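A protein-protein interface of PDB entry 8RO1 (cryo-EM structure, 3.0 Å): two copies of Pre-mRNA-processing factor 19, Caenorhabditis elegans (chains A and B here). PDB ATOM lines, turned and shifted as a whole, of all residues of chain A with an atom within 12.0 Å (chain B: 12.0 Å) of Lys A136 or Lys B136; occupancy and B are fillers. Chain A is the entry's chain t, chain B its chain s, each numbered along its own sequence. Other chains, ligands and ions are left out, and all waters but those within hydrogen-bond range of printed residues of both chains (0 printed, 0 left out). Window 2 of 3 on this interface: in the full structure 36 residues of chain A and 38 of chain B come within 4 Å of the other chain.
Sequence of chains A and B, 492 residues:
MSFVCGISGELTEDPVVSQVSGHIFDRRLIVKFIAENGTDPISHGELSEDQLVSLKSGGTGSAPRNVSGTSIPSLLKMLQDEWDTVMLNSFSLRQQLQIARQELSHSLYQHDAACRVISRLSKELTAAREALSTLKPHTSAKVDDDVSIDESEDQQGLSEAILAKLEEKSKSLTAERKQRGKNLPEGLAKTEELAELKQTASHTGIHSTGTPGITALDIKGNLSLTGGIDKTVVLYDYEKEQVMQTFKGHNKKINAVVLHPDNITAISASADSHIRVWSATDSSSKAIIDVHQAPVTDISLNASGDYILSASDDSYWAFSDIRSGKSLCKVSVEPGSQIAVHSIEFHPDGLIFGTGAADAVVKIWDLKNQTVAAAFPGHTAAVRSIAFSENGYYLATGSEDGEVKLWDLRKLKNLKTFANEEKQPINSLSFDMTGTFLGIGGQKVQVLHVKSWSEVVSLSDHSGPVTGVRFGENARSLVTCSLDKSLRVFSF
Ala A128 touches Ala B128 (CB to CB, 3.7 Å).
Ala A128 touches Leu B132.
CD2 of Leu B132 touches CB of Ala A131 (3.7 Å).
Leu A132 touches Ala B131 (CD1 to CB, 3.9 Å).
Leu B132 touches Leu A132.
CD2 of Leu A132 touches CD1 of Leu B135, 3.97 Å away.
Leu A135 touches Leu B135.
Lys A136 touches Lys B136 (NZ to O, 3.9 Å).
Lys A136 touches one residue of chain B.
Of chain A, only Lys A136 comes within 4 Å of Lys B136.
No residue of chain B comes within 4 Å of Thr A134.
Leu A135 touches just one residue of chain B: Leu B135.
No residue of chain A comes within 4 Å of Thr B134.
Of chain A, only Leu A132 and Leu A135 come within 4 Å of Leu B135.
Pro B137 touches none of the printed residues of chain A.
Printed residues of chain B within 4 Å of Ala A128: Ala B128 and Leu B132.
Of the printed residues of chain A, Ala B131 touches Leu A132.
Of the printed residues of chain A, Leu B132 touches Ala A128 (3.9 Å), Ala A131 (3.7 Å) and Leu A132 (3.8 Å).
Ala A127 touches none of the printed residues of chain B.
Glu B130 touches none of the printed residues of chain A.
Hydrophobic or aromatic side chains of chain A that line the printed part of chain B: Ala A128, Ala A131, Leu A132 and Leu A135.
Among the printed residues, no Asp or Glu carboxylate lies within 4 Å of a Lys or Arg side-chain nitrogen of the other chain.
Ala A128 touches Leu B132, but with the chains exchanged Leu A132 does not touch Ala B128 (4.4 Å).
Leu B132 touches its own counterpart, Leu A132.
Leu A132 touches Leu B135, but with the chains exchanged Leu A135 does not touch Leu B132 (4.3 Å).
Lys A136 touches its own counterpart, Lys B136.
Positions printed for both chains: 127, 128, 129, 130, 131, 132, 133, 134, 135, 136 and 137.
Of the 8 pairs that touch across the chains among the printed residues, 6 have their exchanged pair printed and touching as well.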
ATOM      1  N   ALA A 127     -21.205  -8.525  27.994  1.00  0.00           N
ATOM      2  CA  ALA A 127     -21.506  -9.700  28.809  1.00  0.00           C
ATOM      3  C   ALA A 127     -20.525 -10.841  28.564  1.00  0.00           C
ATOM      4  O   ALA A 127     -20.124 -11.532  29.505  1.00  0.00           O
ATOM      5  CB  ALA A 127     -22.933 -10.170  28.544  1.00  0.00           C
ATOM      6  N   ALA A 128     -20.131 -11.065  27.313  1.00  0.00           N
ATOM      7  CA  ALA A 128     -19.169 -12.124  27.024  1.00  0.00           C
ATOM      8  C   ALA A 128     -17.799 -11.798  27.603  1.00  0.00           C
ATOM      9  O   ALA A 128     -17.097 -12.689  28.090  1.00  0.00           O
ATOM     10  CB  ALA A 128     -19.069 -12.356  25.522  1.00  0.00           C
ATOM     11  N   ARG A 129     -17.391 -10.535  27.533  1.00  0.00           N
ATOM     12  CA  ARG A 129     -16.132 -10.116  28.140  1.00  0.00           C
ATOM     13  C   ARG A 129     -16.184 -10.204  29.659  1.00  0.00           C
ATOM     14  O   ARG A 129     -15.179 -10.524  30.299  1.00  0.00           O
ATOM     15  CB  ARG A 129     -15.793  -8.694  27.697  1.00  0.00           C
ATOM     16  CG  ARG A 129     -15.319  -8.622  26.260  1.00  0.00           C
ATOM     17  CD  ARG A 129     -15.034  -7.205  25.809  1.00  0.00           C
ATOM     18  NE  ARG A 129     -14.403  -7.206  24.494  1.00  0.00           N
ATOM     19  CZ  ARG A 129     -14.452  -6.222  23.604  1.00  0.00           C
ATOM     20  NH1 ARG A 129     -13.862  -6.391  22.424  1.00  0.00           N
ATOM     21  NH2 ARG A 129     -15.050  -5.070  23.863  1.00  0.00           N
ATOM     22  N   GLU A 130     -17.335  -9.898  30.255  1.00  0.00           N
ATOM     23  CA  GLU A 130     -17.500 -10.098  31.690  1.00  0.00           C
ATOM     24  C   GLU A 130     -17.498 -11.571  32.087  1.00  0.00           C
ATOM     25  O   GLU A 130     -17.077 -11.900  33.199  1.00  0.00           O
ATOM     26  CB  GLU A 130     -18.785  -9.428  32.171  1.00  0.00           C
ATOM     27  CG  GLU A 130     -18.680  -7.918  32.242  1.00  0.00           C
ATOM     28  CD  GLU A 130     -19.974  -7.258  32.674  1.00  0.00           C
ATOM     29  OE1 GLU A 130     -20.880  -7.974  33.150  1.00  0.00           O
ATOM     30  OE2 GLU A 130     -20.082  -6.022  32.544  1.00  0.00           O
ATOM     31  N   ALA A 131     -17.965 -12.465  31.215  1.00  0.00           N
ATOM     32  CA  ALA A 131     -17.888 -13.895  31.514  1.00  0.00           C
ATOM     33  C   ALA A 131     -16.449 -14.390  31.622  1.00  0.00           C
ATOM     34  O   ALA A 131     -16.131 -15.171  32.523  1.00  0.00           O
ATOM     35  CB  ALA A 131     -18.640 -14.694  30.454  1.00  0.00           C
ATOM     36  N   LEU A 132     -15.568 -13.971  30.712  1.00  0.00           N
ATOM     37  CA  LEU A 132     -14.160 -14.352  30.817  1.00  0.00           C
ATOM     38  C   LEU A 132     -13.541 -13.858  32.118  1.00  0.00           C
ATOM     39  O   LEU A 132     -12.833 -14.602  32.802  1.00  0.00           O
ATOM     40  CB  LEU A 132     -13.366 -13.835  29.623  1.00  0.00           C
ATOM     41  CG  LEU A 132     -13.598 -14.556  28.294  1.00  0.00           C
ATOM     42  CD1 LEU A 132     -13.027 -13.753  27.140  1.00  0.00           C
ATOM     43  CD2 LEU A 132     -12.992 -15.938  28.317  1.00  0.00           C
ATOM     44  N   SER A 133     -13.802 -12.608  32.485  1.00  0.00           N
ATOM     45  CA  SER A 133     -13.273 -12.105  33.746  1.00  0.00           C
ATOM     46  C   SER A 133     -13.965 -12.719  34.953  1.00  0.00           C
ATOM     47  O   SER A 133     -13.468 -12.555  36.071  1.00  0.00           O
ATOM     48  CB  SER A 133     -13.392 -10.584  33.808  1.00  0.00           C
ATOM     49  OG  SER A 133     -14.742 -10.184  33.919  1.00  0.00           O
ATOM     50  N   THR A 134     -15.107 -13.386  34.773  1.00  0.00           N
ATOM     51  CA  THR A 134     -15.694 -14.135  35.875  1.00  0.00           C
ATOM     52  C   THR A 134     -14.962 -15.453  36.095  1.00  0.00           C
ATOM     53  O   THR A 134     -14.869 -15.912  37.238  1.00  0.00           O
ATOM     54  CB  THR A 134     -17.182 -14.376  35.604  1.00  0.00           C
ATOM     55  OG1 THR A 134     -17.851 -13.117  35.493  1.00  0.00           O
ATOM     56  CG2 THR A 134     -17.847 -15.166  36.734  1.00  0.00           C
ATOM     57  N   LEU A 135     -14.438 -16.070  35.032  1.00  0.00           N
ATOM     58  CA  LEU A 135     -13.960 -17.449  35.087  1.00  0.00           C
ATOM     59  C   LEU A 135     -12.455 -17.572  35.250  1.00  0.00           C
ATOM     60  O   LEU A 135     -12.002 -18.357  36.087  1.00  0.00           O
ATOM     61  CB  LEU A 135     -14.356 -18.230  33.835  1.00  0.00           C
ATOM     62  CG  LEU A 135     -15.837 -18.417  33.538  1.00  0.00           C
ATOM     63  CD1 LEU A 135     -15.989 -19.214  32.256  1.00  0.00           C
ATOM     64  CD2 LEU A 135     -16.554 -19.076  34.688  1.00  0.00           C
ATOM     65  N   LYS A 136     -11.664 -16.802  34.512  1.00  0.00           N
ATOM     66  CA  LYS A 136     -10.222 -16.991  34.592  1.00  0.00           C
ATOM     67  C   LYS A 136      -9.648 -16.354  35.858  1.00  0.00           C
ATOM     68  O   LYS A 136      -8.826 -16.997  36.523  1.00  0.00           O
ATOM     69  CB  LYS A 136      -9.529 -16.480  33.325  1.00  0.00           C
ATOM     70  CG  LYS A 136      -8.014 -16.651  33.360  1.00  0.00           C
ATOM     71  CD  LYS A 136      -7.359 -16.470  31.998  1.00  0.00           C
ATOM     72  CE  LYS A 136      -7.497 -17.705  31.125  1.00  0.00           C
ATOM     73  NZ  LYS A 136      -6.374 -18.651  31.350  1.00  0.00           N
ATOM     74  N   PRO A 137      -9.995 -15.103  36.219  1.00  0.00           N
ATOM     75  CA  PRO A 137      -9.505 -14.643  37.528  1.00  0.00           C
ATOM     76  C   PRO A 137     -10.029 -15.458  38.710  1.00  0.00           C
ATOM     77  O   PRO A 137     -11.246 -15.577  38.862  1.00  0.00           O
ATOM     78  CB  PRO A 137     -10.033 -13.208  37.612  1.00  0.00           C
ATOM     79  CG  PRO A 137     -10.165 -12.785  36.220  1.00  0.00           C
ATOM     80  CD  PRO A 137     -10.648 -14.003  35.492  1.00  0.00           C
ATOM     81  N   ALA B 127     -15.418 -13.371  18.454  1.00  0.00           N
ATOM     82  CA  ALA B 127     -14.133 -13.649  19.084  1.00  0.00           C
ATOM     83  C   ALA B 127     -14.275 -13.830  20.586  1.00  0.00           C
ATOM     84  O   ALA B 127     -13.593 -14.672  21.179  1.00  0.00           O
ATOM     85  CB  ALA B 127     -13.144 -12.531  18.782  1.00  0.00           C
ATOM     86  N   ALA B 128     -15.134 -13.043  21.226  1.00  0.00           N
ATOM     87  CA  ALA B 128     -15.350 -13.220  22.656  1.00  0.00           C
ATOM     88  C   ALA B 128     -16.023 -14.553  22.953  1.00  0.00           C
ATOM     89  O   ALA B 128     -15.604 -15.277  23.861  1.00  0.00           O
ATOM     90  CB  ALA B 128     -16.182 -12.063  23.206  1.00  0.00           C
ATOM     91  N   ARG B 129     -17.060 -14.907  22.198  1.00  0.00           N
ATOM     92  CA  ARG B 129     -17.698 -16.202  22.411  1.00  0.00           C
ATOM     93  C   ARG B 129     -16.808 -17.370  22.020  1.00  0.00           C
ATOM     94  O   ARG B 129     -16.958 -18.464  22.570  1.00  0.00           O
ATOM     95  CB  ARG B 129     -19.006 -16.297  21.639  1.00  0.00           C
ATOM     96  CG  ARG B 129     -20.111 -15.483  22.235  1.00  0.00           C
ATOM     97  CD  ARG B 129     -21.472 -15.996  21.853  1.00  0.00           C
ATOM     98  NE  ARG B 129     -22.469 -15.296  22.648  1.00  0.00           N
ATOM     99  CZ  ARG B 129     -23.585 -15.819  23.135  1.00  0.00           C
ATOM    100  NH1 ARG B 129     -24.318 -15.096  23.974  1.00  0.00           N
ATOM    101  NH2 ARG B 129     -24.006 -17.030  22.794  1.00  0.00           N
ATOM    102  N   GLU B 130     -15.905 -17.184  21.065  1.00  0.00           N
ATOM    103  CA  GLU B 130     -14.940 -18.232  20.753  1.00  0.00           C
ATOM    104  C   GLU B 130     -13.979 -18.457  21.913  1.00  0.00           C
ATOM    105  O   GLU B 130     -13.635 -19.599  22.228  1.00  0.00           O
ATOM    106  CB  GLU B 130     -14.190 -17.865  19.473  1.00  0.00           C
ATOM    107  CG  GLU B 130     -13.125 -18.845  18.984  1.00  0.00           C
ATOM    108  CD  GLU B 130     -13.728 -20.035  18.267  1.00  0.00           C
ATOM    109  OE1 GLU B 130     -14.848 -20.450  18.624  1.00  0.00           O
ATOM    110  OE2 GLU B 130     -13.083 -20.553  17.332  1.00  0.00           O
ATOM    111  N   ALA B 131     -13.527 -17.377  22.551  1.00  0.00           N
ATOM    112  CA  ALA B 131     -12.652 -17.503  23.711  1.00  0.00           C
ATOM    113  C   ALA B 131     -13.331 -18.245  24.852  1.00  0.00           C
ATOM    114  O   ALA B 131     -12.694 -19.044  25.543  1.00  0.00           O
ATOM    115  CB  ALA B 131     -12.196 -16.125  24.179  1.00  0.00           C
ATOM    116  N   LEU B 132     -14.621 -17.996  25.068  1.00  0.00           N
ATOM    117  CA  LEU B 132     -15.374 -18.774  26.044  1.00  0.00           C
ATOM    118  C   LEU B 132     -15.505 -20.232  25.624  1.00  0.00           C
ATOM    119  O   LEU B 132     -15.268 -21.140  26.425  1.00  0.00           O
ATOM    120  CB  LEU B 132     -16.753 -18.159  26.247  1.00  0.00           C
ATOM    121  CG  LEU B 132     -16.845 -16.875  27.067  1.00  0.00           C
ATOM    122  CD1 LEU B 132     -18.193 -16.223  26.853  1.00  0.00           C
ATOM    123  CD2 LEU B 132     -16.620 -17.122  28.544  1.00  0.00           C
ATOM    124  N   SER B 133     -15.876 -20.479  24.369  1.00  0.00           N
ATOM    125  CA  SER B 133     -16.125 -21.840  23.904  1.00  0.00           C
ATOM    126  C   SER B 133     -14.878 -22.719  23.881  1.00  0.00           C
ATOM    127  O   SER B 133     -15.018 -23.941  23.807  1.00  0.00           O
ATOM    128  CB  SER B 133     -16.748 -21.806  22.516  1.00  0.00           C
ATOM    129  OG  SER B 133     -17.996 -21.138  22.543  1.00  0.00           O
ATOM    130  N   THR B 134     -13.679 -22.135  23.899  1.00  0.00           N
ATOM    131  CA  THR B 134     -12.422 -22.881  23.912  1.00  0.00           C
ATOM    132  C   THR B 134     -11.596 -22.583  25.156  1.00  0.00           C
ATOM    133  O   THR B 134     -10.393 -22.850  25.172  1.00  0.00           O
ATOM    134  CB  THR B 134     -11.601 -22.577  22.661  1.00  0.00           C
ATOM    135  OG1 THR B 134     -11.286 -21.181  22.619  1.00  0.00           O
ATOM    136  CG2 THR B 134     -12.355 -22.967  21.407  1.00  0.00           C
ATOM    137  N   LEU B 135     -12.211 -22.020  26.192  1.00  0.00           N
ATOM    138  CA  LEU B 135     -11.480 -21.576  27.369  1.00  0.00           C
ATOM    139  C   LEU B 135     -10.869 -22.779  28.081  1.00  0.00           C
ATOM    140  O   LEU B 135     -11.592 -23.681  28.517  1.00  0.00           O
ATOM    141  CB  LEU B 135     -12.429 -20.814  28.286  1.00  0.00           C
ATOM    142  CG  LEU B 135     -11.913 -20.205  29.574  1.00  0.00           C
ATOM    143  CD1 LEU B 135     -10.876 -19.153  29.273  1.00  0.00           C
ATOM    144  CD2 LEU B 135     -13.082 -19.588  30.312  1.00  0.00           C
ATOM    145  N   LYS B 136      -9.535 -22.807  28.165  1.00  0.00           N
ATOM    146  CA  LYS B 136      -8.756 -23.786  28.907  1.00  0.00           C
ATOM    147  C   LYS B 136      -7.827 -23.101  29.900  1.00  0.00           C
ATOM    148  O   LYS B 136      -7.331 -22.008  29.611  1.00  0.00           O
ATOM    149  CB  LYS B 136      -7.907 -24.634  27.968  1.00  0.00           C
ATOM    150  CG  LYS B 136      -8.696 -25.577  27.117  1.00  0.00           C
ATOM    151  CD  LYS B 136      -7.771 -26.467  26.324  1.00  0.00           C
ATOM    152  CE  LYS B 136      -8.547 -27.511  25.559  1.00  0.00           C
ATOM    153  NZ  LYS B 136      -7.639 -28.443  24.846  1.00  0.00           N
ATOM    154  N   PRO B 137      -7.575 -23.695  31.081  1.00  0.00           N
ATOM    155  CA  PRO B 137      -6.673 -22.981  31.988  1.00  0.00           C
ATOM    156  C   PRO B 137      -5.235 -22.966  31.471  1.00  0.00           C
ATOM    157  O   PRO B 137      -4.319 -22.602  32.208  1.00  0.00           O
ATOM    158  CB  PRO B 137      -6.777 -23.778  33.288  1.00  0.00           C
ATOM    159  CG  PRO B 137      -7.173 -25.122  32.865  1.00  0.00           C
ATOM    160  CD  PRO B 137      -8.062 -24.946  31.685  1.00  0.00           C
